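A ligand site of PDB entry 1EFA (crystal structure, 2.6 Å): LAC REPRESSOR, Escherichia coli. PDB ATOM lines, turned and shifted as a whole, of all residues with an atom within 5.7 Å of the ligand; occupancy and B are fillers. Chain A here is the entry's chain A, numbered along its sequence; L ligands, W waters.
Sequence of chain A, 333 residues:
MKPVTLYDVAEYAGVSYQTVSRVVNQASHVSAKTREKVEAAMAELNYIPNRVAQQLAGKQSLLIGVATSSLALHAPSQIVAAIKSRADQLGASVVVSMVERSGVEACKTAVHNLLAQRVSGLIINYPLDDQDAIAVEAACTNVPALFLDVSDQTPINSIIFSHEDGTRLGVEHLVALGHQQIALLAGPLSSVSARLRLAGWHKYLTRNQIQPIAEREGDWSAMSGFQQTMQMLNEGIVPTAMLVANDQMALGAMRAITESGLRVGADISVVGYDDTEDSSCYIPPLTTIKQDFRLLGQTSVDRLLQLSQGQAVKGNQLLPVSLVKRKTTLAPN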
ATOM      1  N   LEU A  73      28.210   1.533 -19.177  1.00  0.00           N
ATOM      2  CA  LEU A  73      27.356   2.680 -18.864  1.00  0.00           C
ATOM      3  C   LEU A  73      28.009   3.951 -19.388  1.00  0.00           C
ATOM      4  O   LEU A  73      29.226   4.097 -19.321  1.00  0.00           O
ATOM      5  CB  LEU A  73      27.149   2.778 -17.357  1.00  0.00           C
ATOM      6  CG  LEU A  73      26.434   1.559 -16.773  1.00  0.00           C
ATOM      7  CD1 LEU A  73      26.716   1.469 -15.260  1.00  0.00           C
ATOM      8  CD2 LEU A  73      24.944   1.634 -17.082  1.00  0.00           C
ATOM      9  N   HIS A  74      27.188   4.870 -19.873  1.00  0.00           N
ATOM     10  CA  HIS A  74      27.712   6.100 -20.444  1.00  0.00           C
ATOM     11  C   HIS A  74      28.725   6.881 -19.635  1.00  0.00           C
ATOM     12  O   HIS A  74      29.899   6.933 -20.005  1.00  0.00           O
ATOM     13  CB  HIS A  74      26.572   7.043 -20.830  1.00  0.00           C
ATOM     14  CG  HIS A  74      27.049   8.212 -21.633  1.00  0.00           C
ATOM     15  ND1 HIS A  74      27.511   8.082 -22.931  1.00  0.00           N
ATOM     16  CD2 HIS A  74      27.198   9.514 -21.304  1.00  0.00           C
ATOM     17  CE1 HIS A  74      27.926   9.256 -23.360  1.00  0.00           C
ATOM     18  NE2 HIS A  74      27.751  10.146 -22.396  1.00  0.00           N
ATOM     19  N   ALA A  75      28.298   7.512 -18.552  1.00  0.00           N
ATOM     20  CA  ALA A  75      29.216   8.336 -17.753  1.00  0.00           C
ATOM     21  C   ALA A  75      30.507   7.636 -17.327  1.00  0.00           C
ATOM     22  O   ALA A  75      31.597   8.182 -17.463  1.00  0.00           O
ATOM     23  CB  ALA A  75      28.491   8.891 -16.540  1.00  0.00           C
ATOM     24  N   PRO A  76      30.393   6.417 -16.793  1.00  0.00           N
ATOM     25  CA  PRO A  76      31.612   5.720 -16.383  1.00  0.00           C
ATOM     26  C   PRO A  76      32.612   5.604 -17.540  1.00  0.00           C
ATOM     27  O   PRO A  76      33.810   5.907 -17.369  1.00  0.00           O
ATOM     28  CB  PRO A  76      31.106   4.343 -15.938  1.00  0.00           C
ATOM     29  CG  PRO A  76      29.725   4.633 -15.472  1.00  0.00           C
ATOM     30  CD  PRO A  76      29.192   5.640 -16.478  1.00  0.00           C
ATOM     31  N   ILE A  79      34.205   8.827 -18.226  1.00  0.00           N
ATOM     32  CA  ILE A  79      35.119   9.188 -17.153  1.00  0.00           C
ATOM     33  C   ILE A  79      36.432   8.428 -17.213  1.00  0.00           C
ATOM     34  O   ILE A  79      37.507   9.027 -17.149  1.00  0.00           O
ATOM     35  CB  ILE A  79      34.428   9.022 -15.755  1.00  0.00           C
ATOM     36  CG1 ILE A  79      33.370  10.127 -15.592  1.00  0.00           C
ATOM     37  CG2 ILE A  79      35.452   9.092 -14.617  1.00  0.00           C
ATOM     38  CD1 ILE A  79      32.283   9.784 -14.598  1.00  0.00           C
ATOM     39  N   ASN A 125      35.035   5.138  -8.666  1.00  0.00           N
ATOM     40  CA  ASN A 125      33.868   5.672  -9.341  1.00  0.00           C
ATOM     41  C   ASN A 125      32.838   4.564  -9.246  1.00  0.00           C
ATOM     42  O   ASN A 125      32.574   3.847 -10.227  1.00  0.00           O
ATOM     43  CB  ASN A 125      34.172   5.970 -10.800  1.00  0.00           C
ATOM     44  CG  ASN A 125      32.962   6.494 -11.544  1.00  0.00           C
ATOM     45  OD1 ASN A 125      32.991   6.632 -12.770  1.00  0.00           O
ATOM     46  ND2 ASN A 125      31.895   6.792 -10.811  1.00  0.00           N
ATOM     47  N   LEU A 148      34.161   9.440  -6.569  1.00  0.00           N
ATOM     48  CA  LEU A 148      33.381  10.194  -7.547  1.00  0.00           C
ATOM     49  C   LEU A 148      31.883   9.896  -7.500  1.00  0.00           C
ATOM     50  O   LEU A 148      31.096  10.555  -8.175  1.00  0.00           O
ATOM     51  CB  LEU A 148      33.900   9.919  -8.972  1.00  0.00           C
ATOM     52  CG  LEU A 148      35.400  10.099  -9.218  1.00  0.00           C
ATOM     53  CD1 LEU A 148      35.671   9.969 -10.711  1.00  0.00           C
ATOM     54  CD2 LEU A 148      35.842  11.476  -8.711  1.00  0.00           C
ATOM     55  N   ASP A 149      31.490   8.881  -6.726  1.00  0.00           N
ATOM     56  CA  ASP A 149      30.067   8.559  -6.609  1.00  0.00           C
ATOM     57  C   ASP A 149      29.630   8.406  -5.139  1.00  0.00           C
ATOM     58  O   ASP A 149      29.144   7.346  -4.700  1.00  0.00           O
ATOM     59  CB  ASP A 149      29.733   7.289  -7.387  1.00  0.00           C
ATOM     60  CG  ASP A 149      28.227   7.135  -7.644  1.00  0.00           C
ATOM     61  OD1 ASP A 149      27.465   8.070  -7.289  1.00  0.00           O
ATOM     62  OD2 ASP A 149      27.812   6.097  -8.212  1.00  0.00           O
ATOM     63  N   PHE A 161      29.856  16.532  -9.447  1.00  0.00           N
ATOM     64  CA  PHE A 161      29.287  17.702 -10.060  1.00  0.00           C
ATOM     65  C   PHE A 161      28.317  18.296  -9.048  1.00  0.00           C
ATOM     66  O   PHE A 161      27.749  17.582  -8.222  1.00  0.00           O
ATOM     67  CB  PHE A 161      28.573  17.344 -11.372  1.00  0.00           C
ATOM     68  CG  PHE A 161      29.515  17.100 -12.519  1.00  0.00           C
ATOM     69  CD1 PHE A 161      29.782  15.812 -12.964  1.00  0.00           C
ATOM     70  CD2 PHE A 161      30.192  18.175 -13.117  1.00  0.00           C
ATOM     71  CE1 PHE A 161      30.709  15.580 -13.981  1.00  0.00           C
ATOM     72  CE2 PHE A 161      31.129  17.950 -14.126  1.00  0.00           C
ATOM     73  CZ  PHE A 161      31.388  16.645 -14.559  1.00  0.00           C
ATOM     74  N   SER A 191      21.683   4.364  -6.627  1.00  0.00           N
ATOM     75  CA  SER A 191      22.745   5.267  -7.069  1.00  0.00           C
ATOM     76  C   SER A 191      22.819   6.550  -6.230  1.00  0.00           C
ATOM     77  O   SER A 191      21.842   7.290  -6.121  1.00  0.00           O
ATOM     78  CB  SER A 191      22.549   5.639  -8.547  1.00  0.00           C
ATOM     79  OG  SER A 191      23.366   6.739  -8.908  1.00  0.00           O
ATOM     80  N   SER A 193      24.438   9.303  -6.852  1.00  0.00           N
ATOM     81  CA  SER A 193      24.242  10.438  -7.734  1.00  0.00           C
ATOM     82  C   SER A 193      22.751  10.642  -8.042  1.00  0.00           C
ATOM     83  O   SER A 193      22.254  11.775  -8.065  1.00  0.00           O
ATOM     84  CB  SER A 193      25.023  10.220  -9.032  1.00  0.00           C
ATOM     85  OG  SER A 193      25.109  11.431  -9.751  1.00  0.00           O
ATOM     86  N   ARG A 197      20.436  13.977  -7.000  1.00  0.00           N
ATOM     87  CA  ARG A 197      19.625  14.778  -7.914  1.00  0.00           C
ATOM     88  C   ARG A 197      18.187  14.817  -7.432  1.00  0.00           C
ATOM     89  O   ARG A 197      17.536  15.861  -7.477  1.00  0.00           O
ATOM     90  CB  ARG A 197      19.708  14.216  -9.340  1.00  0.00           C
ATOM     91  CG  ARG A 197      21.094  14.339  -9.963  1.00  0.00           C
ATOM     92  CD  ARG A 197      21.226  13.613 -11.297  1.00  0.00           C
ATOM     93  NE  ARG A 197      22.626  13.329 -11.563  1.00  0.00           N
ATOM     94  CZ  ARG A 197      23.089  12.576 -12.564  1.00  0.00           C
ATOM     95  NH1 ARG A 197      22.255  12.015 -13.415  1.00  0.00           N
ATOM     96  NH2 ARG A 197      24.400  12.365 -12.673  1.00  0.00           N
ATOM     97  N   TRP A 220      18.312   4.444 -15.462  1.00  0.00           N
ATOM     98  CA  TRP A 220      19.264   5.119 -16.337  1.00  0.00           C
ATOM     99  C   TRP A 220      18.996   4.841 -17.816  1.00  0.00           C
ATOM    100  O   TRP A 220      19.344   5.654 -18.661  1.00  0.00           O
ATOM    101  CB  TRP A 220      20.696   4.693 -16.008  1.00  0.00           C
ATOM    102  CG  TRP A 220      21.211   5.153 -14.680  1.00  0.00           C
ATOM    103  CD1 TRP A 220      21.963   4.425 -13.811  1.00  0.00           C
ATOM    104  CD2 TRP A 220      21.164   6.494 -14.156  1.00  0.00           C
ATOM    105  NE1 TRP A 220      22.412   5.224 -12.788  1.00  0.00           N
ATOM    106  CE2 TRP A 220      21.936   6.493 -12.968  1.00  0.00           C
ATOM    107  CE3 TRP A 220      20.563   7.687 -14.572  1.00  0.00           C
ATOM    108  CZ2 TRP A 220      22.129   7.651 -12.194  1.00  0.00           C
ATOM    109  CZ3 TRP A 220      20.756   8.846 -13.798  1.00  0.00           C
ATOM    110  CH2 TRP A 220      21.530   8.811 -12.621  1.00  0.00           C
ATOM    111  N   ALA A 245      16.432  12.417 -14.564  1.00  0.00           N
ATOM    112  CA  ALA A 245      17.782  12.213 -14.054  1.00  0.00           C
ATOM    113  C   ALA A 245      18.913  12.163 -15.082  1.00  0.00           C
ATOM    114  O   ALA A 245      20.071  12.434 -14.734  1.00  0.00           O
ATOM    115  CB  ALA A 245      17.797  10.976 -13.173  1.00  0.00           C
ATOM    116  N   ASN A 246      18.606  11.788 -16.321  1.00  0.00           N
ATOM    117  CA  ASN A 246      19.624  11.754 -17.376  1.00  0.00           C
ATOM    118  C   ASN A 246      18.996  11.829 -18.771  1.00  0.00           C
ATOM    119  O   ASN A 246      17.783  11.595 -18.934  1.00  0.00           O
ATOM    120  CB  ASN A 246      20.517  10.513 -17.247  1.00  0.00           C
ATOM    121  CG  ASN A 246      19.836   9.246 -17.705  1.00  0.00           C
ATOM    122  OD1 ASN A 246      18.617   9.197 -17.860  1.00  0.00           O
ATOM    123  ND2 ASN A 246      20.637   8.189 -17.912  1.00  0.00           N
ATOM    124  N   ASP A 247      19.823  12.156 -19.759  1.00  0.00           N
ATOM    125  CA  ASP A 247      19.361  12.300 -21.141  1.00  0.00           C
ATOM    126  C   ASP A 247      18.737  11.033 -21.673  1.00  0.00           C
ATOM    127  O   ASP A 247      17.706  11.083 -22.334  1.00  0.00           O
ATOM    128  CB  ASP A 247      20.515  12.736 -22.028  1.00  0.00           C
ATOM    129  CG  ASP A 247      21.027  14.140 -21.693  1.00  0.00           C
ATOM    130  OD1 ASP A 247      22.172  14.476 -22.121  1.00  0.00           O
ATOM    131  OD2 ASP A 247      20.274  14.916 -21.023  1.00  0.00           O
ATOM    132  N   GLN A 248      19.328   9.890 -21.386  1.00  0.00           N
ATOM    133  CA  GLN A 248      18.772   8.661 -21.897  1.00  0.00           C
ATOM    134  C   GLN A 248      17.360   8.412 -21.429  1.00  0.00           C
ATOM    135  O   GLN A 248      16.503   8.015 -22.231  1.00  0.00           O
ATOM    136  CB  GLN A 248      19.679   7.496 -21.560  1.00  0.00           C
ATOM    137  CG  GLN A 248      20.902   7.496 -22.459  1.00  0.00           C
ATOM    138  CD  GLN A 248      22.039   6.674 -21.903  1.00  0.00           C
ATOM    139  OE1 GLN A 248      22.829   7.155 -21.080  1.00  0.00           O
ATOM    140  NE2 GLN A 248      22.140   5.437 -22.354  1.00  0.00           N
ATOM    141  N   TYR A 273      19.560  15.297 -18.033  1.00  0.00           N
ATOM    142  CA  TYR A 273      20.766  15.496 -17.247  1.00  0.00           C
ATOM    143  C   TYR A 273      21.936  14.771 -17.922  1.00  0.00           C
ATOM    144  O   TYR A 273      21.803  13.598 -18.301  1.00  0.00           O
ATOM    145  CB  TYR A 273      20.494  14.936 -15.834  1.00  0.00           C
ATOM    146  CG  TYR A 273      21.098  15.748 -14.691  1.00  0.00           C
ATOM    147  CD1 TYR A 273      22.444  15.607 -14.359  1.00  0.00           C
ATOM    148  CD2 TYR A 273      20.323  16.689 -13.985  1.00  0.00           C
ATOM    149  CE1 TYR A 273      23.025  16.385 -13.353  1.00  0.00           C
ATOM    150  CE2 TYR A 273      20.893  17.473 -12.985  1.00  0.00           C
ATOM    151  CZ  TYR A 273      22.239  17.314 -12.677  1.00  0.00           C
ATOM    152  OH  TYR A 273      22.854  18.123 -11.734  1.00  0.00           O
ATOM    153  N   ASP A 274      23.060  15.480 -18.083  1.00  0.00           N
ATOM    154  CA  ASP A 274      24.301  14.983 -18.707  1.00  0.00           C
ATOM    155  C   ASP A 274      24.779  15.858 -19.852  1.00  0.00           C
ATOM    156  O   ASP A 274      25.935  16.271 -19.908  1.00  0.00           O
ATOM    157  CB  ASP A 274      24.158  13.587 -19.319  1.00  0.00           C
ATOM    158  CG  ASP A 274      24.230  12.447 -18.309  1.00  0.00           C
ATOM    159  OD1 ASP A 274      24.599  12.676 -17.120  1.00  0.00           O
ATOM    160  OD2 ASP A 274      23.901  11.312 -18.722  1.00  0.00           O
ATOM    161  N   GLN A 291      27.172  18.103 -17.897  1.00  0.00           N
ATOM    162  CA  GLN A 291      28.170  17.575 -16.977  1.00  0.00           C
ATOM    163  C   GLN A 291      29.399  17.215 -17.798  1.00  0.00           C
ATOM    164  O   GLN A 291      29.441  16.179 -18.471  1.00  0.00           O
ATOM    165  CB  GLN A 291      27.665  16.323 -16.274  1.00  0.00           C
ATOM    166  CG  GLN A 291      26.453  16.525 -15.380  1.00  0.00           C
ATOM    167  CD  GLN A 291      26.274  15.338 -14.453  1.00  0.00           C
ATOM    168  OE1 GLN A 291      26.494  15.445 -13.248  1.00  0.00           O
ATOM    169  NE2 GLN A 291      25.898  14.197 -15.028  1.00  0.00           N
ATOM    170  N   PHE A 293      32.209  15.509 -18.428  1.00  0.00           N
ATOM    171  CA  PHE A 293      32.970  14.347 -17.982  1.00  0.00           C
ATOM    172  C   PHE A 293      34.468  14.444 -18.202  1.00  0.00           C
ATOM    173  O   PHE A 293      35.258  13.915 -17.412  1.00  0.00           O
ATOM    174  CB  PHE A 293      32.417  13.109 -18.651  1.00  0.00           C
ATOM    175  CG  PHE A 293      30.963  12.880 -18.378  1.00  0.00           C
ATOM    176  CD1 PHE A 293      30.045  12.909 -19.426  1.00  0.00           C
ATOM    177  CD2 PHE A 293      30.515  12.634 -17.090  1.00  0.00           C
ATOM    178  CE1 PHE A 293      28.681  12.682 -19.165  1.00  0.00           C
ATOM    179  CE2 PHE A 293      29.171  12.409 -16.830  1.00  0.00           C
ATOM    180  CZ  PHE A 293      28.254  12.436 -17.864  1.00  0.00           C
ATOM    181  N   LEU A 296      35.850  16.176 -15.270  1.00  0.00           N
ATOM    182  CA  LEU A 296      35.853  15.343 -14.070  1.00  0.00           C
ATOM    183  C   LEU A 296      37.045  14.388 -14.082  1.00  0.00           C
ATOM    184  O   LEU A 296      37.784  14.310 -13.100  1.00  0.00           O
ATOM    185  CB  LEU A 296      34.543  14.560 -13.956  1.00  0.00           C
ATOM    186  CG  LEU A 296      34.511  13.507 -12.852  1.00  0.00           C
ATOM    187  CD1 LEU A 296      34.664  14.199 -11.510  1.00  0.00           C
ATOM    188  CD2 LEU A 296      33.194  12.701 -12.911  1.00  0.00           C
HETATM  189  C1  LIG L   1      25.460   8.004 -14.567  1.00  0.00           C
HETATM  190  C2  LIG L   1      25.864   6.650 -14.372  1.00  0.00           C
HETATM  191  C3  LIG L   1      25.530   5.573 -15.214  1.00  0.00           C
HETATM  192  C4  LIG L   1      24.735   5.865 -16.338  1.00  0.00           C
HETATM  193  C5  LIG L   1      24.291   7.187 -16.584  1.00  0.00           C
HETATM  194  C6  LIG L   1      24.638   8.259 -15.701  1.00  0.00           C
HETATM  195  N1  LIG L   1      24.143   9.543 -16.020  1.00  0.00           N
HETATM  196  O1  LIG L   1      24.396  10.548 -15.354  1.00  0.00           O
HETATM  197  O2  LIG L   1      23.435   9.614 -17.033  1.00  0.00           O
HETATM  198  O3  LIG L   1      26.353   9.078 -14.244  1.00  0.00           O
HETATM  199  C7  LIG L   1      26.692   9.679 -12.967  1.00  0.00           C
HETATM  200  C8  LIG L   1      27.520   8.865 -11.928  1.00  0.00           C
HETATM  201  O4  LIG L   1      26.718   7.918 -11.179  1.00  0.00           O
HETATM  202  C9  LIG L   1      28.244   9.738 -10.905  1.00  0.00           C
HETATM  203  O5  LIG L   1      29.018   8.852 -10.078  1.00  0.00           O
HETATM  204  C10 LIG L   1      29.154  10.733 -11.627  1.00  0.00           C
HETATM  205  O6  LIG L   1      30.160   9.939 -12.264  1.00  0.00           O
HETATM  206  C11 LIG L   1      28.315  11.570 -12.620  1.00  0.00           C
HETATM  207  C12 LIG L   1      29.230  12.463 -13.439  1.00  0.00           C
HETATM  208  O7  LIG L   1      27.523  10.746 -13.504  1.00  0.00           O
HETATM  209  O   HOH W   1      23.864   5.198 -19.381  1.00  0.00           O
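CB of Leu 73 touches C3 of the ligand, 3.9 Å away.
Ala 75 touches the ligand (CB to O3, 3.1 Å).
Pro 76 touches the ligand (CD to C3, 3.9 Å).
Ile 79 touches the ligand (CD1 to O6, 3.2 Å).
ND2 of Asn 125 touches O5 of the ligand, at 3.6 Å.
Phe 161 touches the ligand (CD1 to C12, 3.4 Å).
Ser 193 touches the ligand (CB to O4, 3.6 Å).
CG of Trp 220 touches C4 of the ligand, 3.96 Å away.
Gln 291 touches the ligand (NE2 to O1, 3.96 Å).
Phe 293 touches the ligand (CE2 to C12, 3.4 Å).
Hydrophobic or aromatic side chains within 4 Å of the ligand: Leu 73, Ala 75, Pro 76, Ile 79, Phe 161, Trp 220 and Phe 293.
The nearest printed residue that does not touch the ligand is Leu 296 (4.01 Å).
Water W1 bridges OE1 of Gln 248 and N of His 74.
OD1 of Asp 149 lies within hydrogen-bond range of N of Ser 193 (3.3 Å).
The guanidinium group (NH2) of Arg 197 lies close to the side-chain amide nitrogen (NE2) of Gln 291 (3.3 Å).
The guanidinium group (NH2) of Arg 197 is in hydrogen-bond range of the side-chain hydroxyl (OG) of Ser 193 (3.1 Å).
The backbone NH of Ser 193 sits close to the side-chain hydroxyl of Ser 191.
The side-chain amide nitrogen of Gln 291 is in hydrogen-bond range of the side-chain carboxylate of Asp 274 (2.9 Å).
The side-chain amide nitrogen (ND2) of Asn 246 sits at hydrogen-bond distance from the backbone carbonyl oxygen (O) of Trp 220 (2.9 Å).
The backbone carbonyl oxygen of Ala 245 sits at hydrogen-bond distance from the guanidinium group of Arg 197, 2.6 Å away.
An oxygen (O5) of the ligand lies within hydrogen-bond range of the backbone carbonyl oxygen (O) of Leu 148, at 3.3 Å.
An oxygen (O2) of the ligand lies close to the side-chain carboxylate (OD2) of Asp 274 (2.4 Å).
ND2 of Asn 246 lies close to O2 of the ligand (3.3 Å).
An oxygen (O1) of the ligand sits at hydrogen-bond distance from the guanidinium group of Arg 197, 3.2 Å away.
The side-chain carboxylate (OD1) of Asp 149 sits close to an oxygen (O5) of the ligand (3.3 Å).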
